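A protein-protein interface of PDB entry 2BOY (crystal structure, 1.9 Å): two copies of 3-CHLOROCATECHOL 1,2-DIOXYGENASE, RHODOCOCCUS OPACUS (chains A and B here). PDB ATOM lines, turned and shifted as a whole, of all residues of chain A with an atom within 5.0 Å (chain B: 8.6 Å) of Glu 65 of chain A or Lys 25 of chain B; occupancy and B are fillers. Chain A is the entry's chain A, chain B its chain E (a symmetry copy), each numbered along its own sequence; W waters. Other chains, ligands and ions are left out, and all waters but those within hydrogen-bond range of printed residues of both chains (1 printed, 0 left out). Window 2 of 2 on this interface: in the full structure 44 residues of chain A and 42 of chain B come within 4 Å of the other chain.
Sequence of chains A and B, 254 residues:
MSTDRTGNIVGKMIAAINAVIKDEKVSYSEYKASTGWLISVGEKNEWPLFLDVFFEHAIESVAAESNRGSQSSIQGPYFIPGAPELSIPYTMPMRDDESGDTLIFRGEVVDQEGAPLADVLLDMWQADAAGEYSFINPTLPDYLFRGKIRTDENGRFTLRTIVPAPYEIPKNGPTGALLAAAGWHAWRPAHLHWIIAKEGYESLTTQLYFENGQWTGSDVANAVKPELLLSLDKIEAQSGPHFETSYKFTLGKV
NH1 of Arg 5 of chain A sits at hydrogen-bond distance from O of Glu 24 of chain B, at 3.0 Å.
NH2 of Arg 5 of chain A lies within hydrogen-bond range of O of Lys 25 of chain B, 3.2 Å away.
The side-chain carboxylate (OE2) of Glu 30 of chain B is in salt-bridge range of the guanidinium group (NE) of Arg 5 of chain A, at 2.8 Å.
The side-chain carboxylate (OE1) of Glu 65 of chain A is in salt-bridge range of the side-chain amino group (NZ) of Lys 25 of chain B, at 3.1 Å.
The backbone carbonyl oxygen of Ile 21 of chain B is in hydrogen-bond range of the backbone NH of Val 26 of chain B.
OE1 of Glu 30 of chain B lies within hydrogen-bond range of N of Ser 27 of chain B, at 2.9 Å.
Among the printed residues, pairs that only touch across the chains: Arg 5 of chain A with Val 26 of chain B, Val 62 of chain A with Ile 21 of chain B, Val 62 of chain A with Lys 25 of chain B, Val 62 of chain A with Val 26 of chain B and Ala 63 of chain A with Tyr 28 of chain B.
No residue of chain B comes within 4 Å of Ala 64 of chain A.
Printed residues of chain B within 4 Å of Val 62 of chain A: Ile 21 (3.8 Å), Lys 25 (3.8 Å) and Val 26 (3.6 Å).
Printed residues of chain B within 4 Å of Ala 63 of chain A: Tyr 28 (3.95 Å).
The nearest printed residue of chain B that does not touch Glu 65 of chain A is Lys 22 of chain B (5.7 Å).
The nearest printed residue of chain A that does not touch Lys 25 of chain B is Ala 63 of chain A (6.9 Å).
The nearest printed residue of chain A that does not touch Val 26 of chain B is Ala 63 of chain A (5.5 Å).
Printed residues of chain B that touch a printed residue of chain A: Ile 21, Glu 24, Lys 25, Val 26, Tyr 28 and Glu 30.
Hydrophobic or aromatic side chains of chain B within 4 Å of the printed part of chain A: Tyr 28.
Of the 8 printed residues of chain A, 4 touch a printed residue of chain B.
Hydrophobic or aromatic side chains of chain A within 4 Å of the printed part of chain B: Val 62 and Ala 63.
Along chain A the printed residues that touch a printed residue of chain B span positions 5 to 65.
No position is printed for both chains.
Of the 9 pairs that touch across the chains among the printed residues, none has its exchanged pair printed and touching as well.
Water W1 lies within hydrogen-bond range of the backbone carbonyl oxygen of Val 26 of chain B (2.8 Å), the backbone NH of Ala 63 of chain A (3.4 Å) and the backbone NH of Tyr 28 of chain B (3.5 Å).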
ATOM      1  N   ARG A   5      -4.606  14.373  13.095  1.00  0.00           N
ATOM      2  CA  ARG A   5      -3.679  14.428  11.972  1.00  0.00           C
ATOM      3  C   ARG A   5      -3.887  13.212  11.057  1.00  0.00           C
ATOM      4  O   ARG A   5      -4.072  13.357   9.826  1.00  0.00           O
ATOM      5  CB  ARG A   5      -2.249  14.438  12.509  1.00  0.00           C
ATOM      6  CG  ARG A   5      -1.218  14.330  11.399  1.00  0.00           C
ATOM      7  CD  ARG A   5       0.136  14.786  11.783  1.00  0.00           C
ATOM      8  NE  ARG A   5       1.106  14.499  10.721  1.00  0.00           N
ATOM      9  CZ  ARG A   5       1.373  15.281   9.693  1.00  0.00           C
ATOM     10  NH1 ARG A   5       0.756  16.463   9.530  1.00  0.00           N
ATOM     11  NH2 ARG A   5       2.310  14.881   8.819  1.00  0.00           N
ATOM     12  N   SER A  61      10.782  14.809  -0.643  1.00  0.00           N
ATOM     13  CA  SER A  61      10.754  16.230  -0.960  1.00  0.00           C
ATOM     14  C   SER A  61      10.322  17.059   0.281  1.00  0.00           C
ATOM     15  O   SER A  61      10.884  18.120   0.537  1.00  0.00           O
ATOM     16  CB  SER A  61       9.809  16.483  -2.119  1.00  0.00           C
ATOM     17  OG  SER A  61       9.737  17.873  -2.375  1.00  0.00           O
ATOM     18  N   VAL A  62       9.388  16.561   1.086  1.00  0.00           N
ATOM     19  CA  VAL A  62       9.070  17.319   2.319  1.00  0.00           C
ATOM     20  C   VAL A  62      10.209  17.250   3.351  1.00  0.00           C
ATOM     21  O   VAL A  62      10.539  18.258   3.993  1.00  0.00           O
ATOM     22  CB  VAL A  62       7.656  17.050   2.980  1.00  0.00           C
ATOM     23  CG1 VAL A  62       6.772  16.196   2.179  1.00  0.00           C
ATOM     24  CG2 VAL A  62       7.738  16.649   4.456  1.00  0.00           C
ATOM     25  N   ALA A  63      10.792  16.068   3.497  1.00  0.00           N
ATOM     26  CA  ALA A  63      11.947  15.861   4.378  1.00  0.00           C
ATOM     27  C   ALA A  63      13.106  16.783   3.985  1.00  0.00           C
ATOM     28  O   ALA A  63      13.796  17.357   4.867  1.00  0.00           O
ATOM     29  CB  ALA A  63      12.398  14.400   4.306  1.00  0.00           C
ATOM     30  N   ALA A  64      13.278  16.961   2.673  1.00  0.00           N
ATOM     31  CA  ALA A  64      14.415  17.685   2.131  1.00  0.00           C
ATOM     32  C   ALA A  64      14.383  19.179   2.489  1.00  0.00           C
ATOM     33  O   ALA A  64      15.444  19.781   2.599  1.00  0.00           O
ATOM     34  CB  ALA A  64      14.540  17.503   0.603  1.00  0.00           C
ATOM     35  N   GLU A  65      13.188  19.745   2.673  1.00  0.00           N
ATOM     36  CA  GLU A  65      13.084  21.143   3.115  1.00  0.00           C
ATOM     37  C   GLU A  65      13.858  21.477   4.417  1.00  0.00           C
ATOM     38  O   GLU A  65      14.236  22.638   4.625  1.00  0.00           O
ATOM     39  CB  GLU A  65      11.641  21.675   3.227  1.00  0.00           C
ATOM     40  CG  GLU A  65      10.487  21.084   2.435  1.00  0.00           C
ATOM     41  CD  GLU A  65       9.153  21.643   2.938  1.00  0.00           C
ATOM     42  OE1 GLU A  65       8.286  20.865   3.402  1.00  0.00           O
ATOM     43  OE2 GLU A  65       8.970  22.882   2.907  1.00  0.00           O
ATOM     44  N   SER A  66      14.132  20.468   5.234  1.00  0.00           N
ATOM     45  CA  SER A  66      14.901  20.617   6.467  1.00  0.00           C
ATOM     46  C   SER A  66      16.381  20.233   6.361  1.00  0.00           C
ATOM     47  O   SER A  66      17.033  20.098   7.385  1.00  0.00           O
ATOM     48  CB  SER A  66      14.290  19.748   7.583  1.00  0.00           C
ATOM     49  OG  SER A  66      13.017  20.238   7.959  1.00  0.00           O
ATOM     50  N   ASN A  67      16.883  19.984   5.150  1.00  0.00           N
ATOM     51  CA  ASN A  67      18.288  19.560   4.954  1.00  0.00           C
ATOM     52  C   ASN A  67      19.256  20.592   5.533  1.00  0.00           C
ATOM     53  O   ASN A  67      19.047  21.790   5.322  1.00  0.00           O
ATOM     54  CB  ASN A  67      18.603  19.441   3.450  1.00  0.00           C
ATOM     55  CG  ASN A  67      18.111  18.115   2.852  1.00  0.00           C
ATOM     56  OD1 ASN A  67      17.570  17.258   3.574  1.00  0.00           O
ATOM     57  ND2 ASN A  67      18.247  17.969   1.540  1.00  0.00           N
ATOM     58  N   ASN B  18       0.034  12.182  -3.678  1.00  0.00           N
ATOM     59  CA  ASN B  18       1.229  12.997  -3.492  1.00  0.00           C
ATOM     60  C   ASN B  18       0.919  14.460  -3.125  1.00  0.00           C
ATOM     61  O   ASN B  18       1.668  15.094  -2.409  1.00  0.00           O
ATOM     62  CB  ASN B  18       2.163  12.929  -4.722  1.00  0.00           C
ATOM     63  CG  ASN B  18       2.829  11.552  -4.852  1.00  0.00           C
ATOM     64  OD1 ASN B  18       2.983  11.011  -5.944  1.00  0.00           O
ATOM     65  ND2 ASN B  18       3.194  10.984  -3.731  1.00  0.00           N
ATOM     66  N   ALA B  19      -0.176  14.996  -3.625  1.00  0.00           N
ATOM     67  CA  ALA B  19      -0.522  16.358  -3.194  1.00  0.00           C
ATOM     68  C   ALA B  19      -0.833  16.448  -1.692  1.00  0.00           C
ATOM     69  O   ALA B  19      -0.426  17.395  -0.994  1.00  0.00           O
ATOM     70  CB  ALA B  19      -1.647  16.913  -4.052  1.00  0.00           C
ATOM     71  N   VAL B  20      -1.518  15.453  -1.148  1.00  0.00           N
ATOM     72  CA  VAL B  20      -1.758  15.444   0.305  1.00  0.00           C
ATOM     73  C   VAL B  20      -0.452  15.271   1.126  1.00  0.00           C
ATOM     74  O   VAL B  20      -0.272  15.882   2.197  1.00  0.00           O
ATOM     75  CB  VAL B  20      -2.803  14.317   0.717  1.00  0.00           C
ATOM     76  CG1 VAL B  20      -2.952  14.209   2.228  1.00  0.00           C
ATOM     77  CG2 VAL B  20      -4.178  14.570   0.077  1.00  0.00           C
ATOM     78  N   ILE B  21       0.429  14.384   0.663  1.00  0.00           N
ATOM     79  CA  ILE B  21       1.727  14.208   1.310  1.00  0.00           C
ATOM     80  C   ILE B  21       2.437  15.571   1.407  1.00  0.00           C
ATOM     81  O   ILE B  21       3.008  15.903   2.455  1.00  0.00           O
ATOM     82  CB  ILE B  21       2.623  13.199   0.519  1.00  0.00           C
ATOM     83  CG1 ILE B  21       2.164  11.753   0.757  1.00  0.00           C
ATOM     84  CG2 ILE B  21       4.125  13.367   0.873  1.00  0.00           C
ATOM     85  CD1 ILE B  21       2.799  10.733  -0.176  1.00  0.00           C
ATOM     86  N   LYS B  22       2.414  16.341   0.319  1.00  0.00           N
ATOM     87  CA  LYS B  22       3.117  17.643   0.294  1.00  0.00           C
ATOM     88  C   LYS B  22       2.383  18.650   1.197  1.00  0.00           C
ATOM     89  O   LYS B  22       3.011  19.333   2.012  1.00  0.00           O
ATOM     90  CB  LYS B  22       3.145  18.193  -1.137  1.00  0.00           C
ATOM     91  CG  LYS B  22       3.644  19.640  -1.279  1.00  0.00           C
ATOM     92  CD  LYS B  22       3.787  19.999  -2.745  1.00  0.00           C
ATOM     93  CE  LYS B  22       4.451  21.332  -2.946  1.00  0.00           C
ATOM     94  NZ  LYS B  22       5.410  21.271  -4.092  1.00  0.00           N
ATOM     95  N   ASP B  23       1.065  18.724   1.047  1.00  0.00           N
ATOM     96  CA  ASP B  23       0.241  19.616   1.860  1.00  0.00           C
ATOM     97  C   ASP B  23       0.371  19.355   3.357  1.00  0.00           C
ATOM     98  O   ASP B  23       0.634  20.302   4.116  1.00  0.00           O
ATOM     99  CB  ASP B  23      -1.220  19.550   1.442  1.00  0.00           C
ATOM    100  CG  ASP B  23      -2.094  20.536   2.236  1.00  0.00           C
ATOM    101  OD1 ASP B  23      -2.937  20.080   3.046  1.00  0.00           O
ATOM    102  OD2 ASP B  23      -1.954  21.777   2.128  1.00  0.00           O
ATOM    103  N   GLU B  24       0.219  18.095   3.792  1.00  0.00           N
ATOM    104  CA  GLU B  24       0.307  17.765   5.216  1.00  0.00           C
ATOM    105  C   GLU B  24       1.696  17.504   5.697  1.00  0.00           C
ATOM    106  O   GLU B  24       1.859  17.177   6.882  1.00  0.00           O
ATOM    107  CB  GLU B  24      -0.468  16.493   5.576  1.00  0.00           C
ATOM    108  CG  GLU B  24      -1.600  16.765   6.550  1.00  0.00           C
ATOM    109  CD  GLU B  24      -2.654  17.455   5.774  1.00  0.00           C
ATOM    110  OE1 GLU B  24      -3.594  18.044   6.342  1.00  0.00           O
ATOM    111  OE2 GLU B  24      -2.459  17.381   4.542  1.00  0.00           O
ATOM    112  N   LYS B  25       2.685  17.569   4.788  1.00  0.00           N
ATOM    113  CA  LYS B  25       4.081  17.327   5.181  1.00  0.00           C
ATOM    114  C   LYS B  25       4.203  15.956   5.844  1.00  0.00           C
ATOM    115  O   LYS B  25       4.766  15.777   6.943  1.00  0.00           O
ATOM    116  CB  LYS B  25       4.609  18.474   6.076  1.00  0.00           C
ATOM    117  CG  LYS B  25       4.619  19.856   5.366  1.00  0.00           C
ATOM    118  CD  LYS B  25       5.248  20.950   6.257  1.00  0.00           C
ATOM    119  CE  LYS B  25       5.130  22.345   5.635  1.00  0.00           C
ATOM    120  NZ  LYS B  25       5.814  22.500   4.303  1.00  0.00           N
ATOM    121  N   VAL B  26       3.696  14.935   5.153  1.00  0.00           N
ATOM    122  CA  VAL B  26       3.819  13.582   5.707  1.00  0.00           C
ATOM    123  C   VAL B  26       5.295  13.231   5.894  1.00  0.00           C
ATOM    124  O   VAL B  26       6.109  13.529   5.039  1.00  0.00           O
ATOM    125  CB  VAL B  26       3.061  12.541   4.829  1.00  0.00           C
ATOM    126  CG1 VAL B  26       3.267  11.162   5.360  1.00  0.00           C
ATOM    127  CG2 VAL B  26       1.555  12.892   4.766  1.00  0.00           C
ATOM    128  N   SER B  27       5.633  12.625   7.028  1.00  0.00           N
ATOM    129  CA  SER B  27       7.012  12.383   7.407  1.00  0.00           C
ATOM    130  C   SER B  27       7.474  10.992   6.956  1.00  0.00           C
ATOM    131  O   SER B  27       6.652  10.147   6.578  1.00  0.00           O
ATOM    132  CB  SER B  27       7.176  12.478   8.924  1.00  0.00           C
ATOM    133  OG  SER B  27       6.683  11.321   9.571  1.00  0.00           O
ATOM    134  N   TYR B  28       8.788  10.767   7.000  1.00  0.00           N
ATOM    135  CA  TYR B  28       9.337   9.453   6.693  1.00  0.00           C
ATOM    136  C   TYR B  28       8.869   8.417   7.700  1.00  0.00           C
ATOM    137  O   TYR B  28       8.617   7.251   7.380  1.00  0.00           O
ATOM    138  CB  TYR B  28      10.867   9.516   6.695  1.00  0.00           C
ATOM    139  CG  TYR B  28      11.437   9.420   5.293  1.00  0.00           C
ATOM    140  CD1 TYR B  28      12.198  10.477   4.765  1.00  0.00           C
ATOM    141  CD2 TYR B  28      11.219   8.268   4.494  1.00  0.00           C
ATOM    142  CE1 TYR B  28      12.746  10.403   3.476  1.00  0.00           C
ATOM    143  CE2 TYR B  28      11.762   8.183   3.185  1.00  0.00           C
ATOM    144  CZ  TYR B  28      12.515   9.267   2.692  1.00  0.00           C
ATOM    145  OH  TYR B  28      13.059   9.233   1.431  1.00  0.00           O
ATOM    146  N   SER B  29       8.788   8.852   8.954  1.00  0.00           N
ATOM    147  CA  SER B  29       8.295   8.004  10.000  1.00  0.00           C
ATOM    148  C   SER B  29       6.826   7.556   9.684  1.00  0.00           C
ATOM    149  O   SER B  29       6.483   6.363   9.816  1.00  0.00           O
ATOM    150  CB  SER B  29       8.421   8.773  11.358  1.00  0.00           C
ATOM    151  OG  SER B  29       7.836   8.021  12.380  1.00  0.00           O
ATOM    152  N   GLU B  30       5.992   8.477   9.220  1.00  0.00           N
ATOM    153  CA  GLU B  30       4.597   8.135   8.881  1.00  0.00           C
ATOM    154  C   GLU B  30       4.538   7.208   7.639  1.00  0.00           C
ATOM    155  O   GLU B  30       3.698   6.304   7.560  1.00  0.00           O
ATOM    156  CB  GLU B  30       3.763   9.392   8.659  1.00  0.00           C
ATOM    157  CG  GLU B  30       3.528  10.155   9.967  1.00  0.00           C
ATOM    158  CD  GLU B  30       3.126  11.608   9.826  1.00  0.00           C
ATOM    159  OE1 GLU B  30       3.314  12.257   8.774  1.00  0.00           O
ATOM    160  OE2 GLU B  30       2.549  12.122  10.811  1.00  0.00           O
ATOM    161  N   TYR B  31       5.450   7.458   6.694  1.00  0.00           N
ATOM    162  CA  TYR B  31       5.552   6.641   5.467  1.00  0.00           C
ATOM    163  C   TYR B  31       5.916   5.201   5.810  1.00  0.00           C
ATOM    164  O   TYR B  31       5.326   4.243   5.269  1.00  0.00           O
ATOM    165  CB  TYR B  31       6.630   7.229   4.585  1.00  0.00           C
ATOM    166  CG  TYR B  31       6.901   6.509   3.277  1.00  0.00           C
ATOM    167  CD1 TYR B  31       5.911   6.397   2.303  1.00  0.00           C
ATOM    168  CD2 TYR B  31       8.173   5.951   3.021  1.00  0.00           C
ATOM    169  CE1 TYR B  31       6.178   5.737   1.077  1.00  0.00           C
ATOM    170  CE2 TYR B  31       8.461   5.311   1.789  1.00  0.00           C
ATOM    171  CZ  TYR B  31       7.449   5.208   0.835  1.00  0.00           C
ATOM    172  OH  TYR B  31       7.682   4.603  -0.383  1.00  0.00           O
HETATM  173  O   HOH W   1       8.939  13.539   4.898  1.00  0.00           O
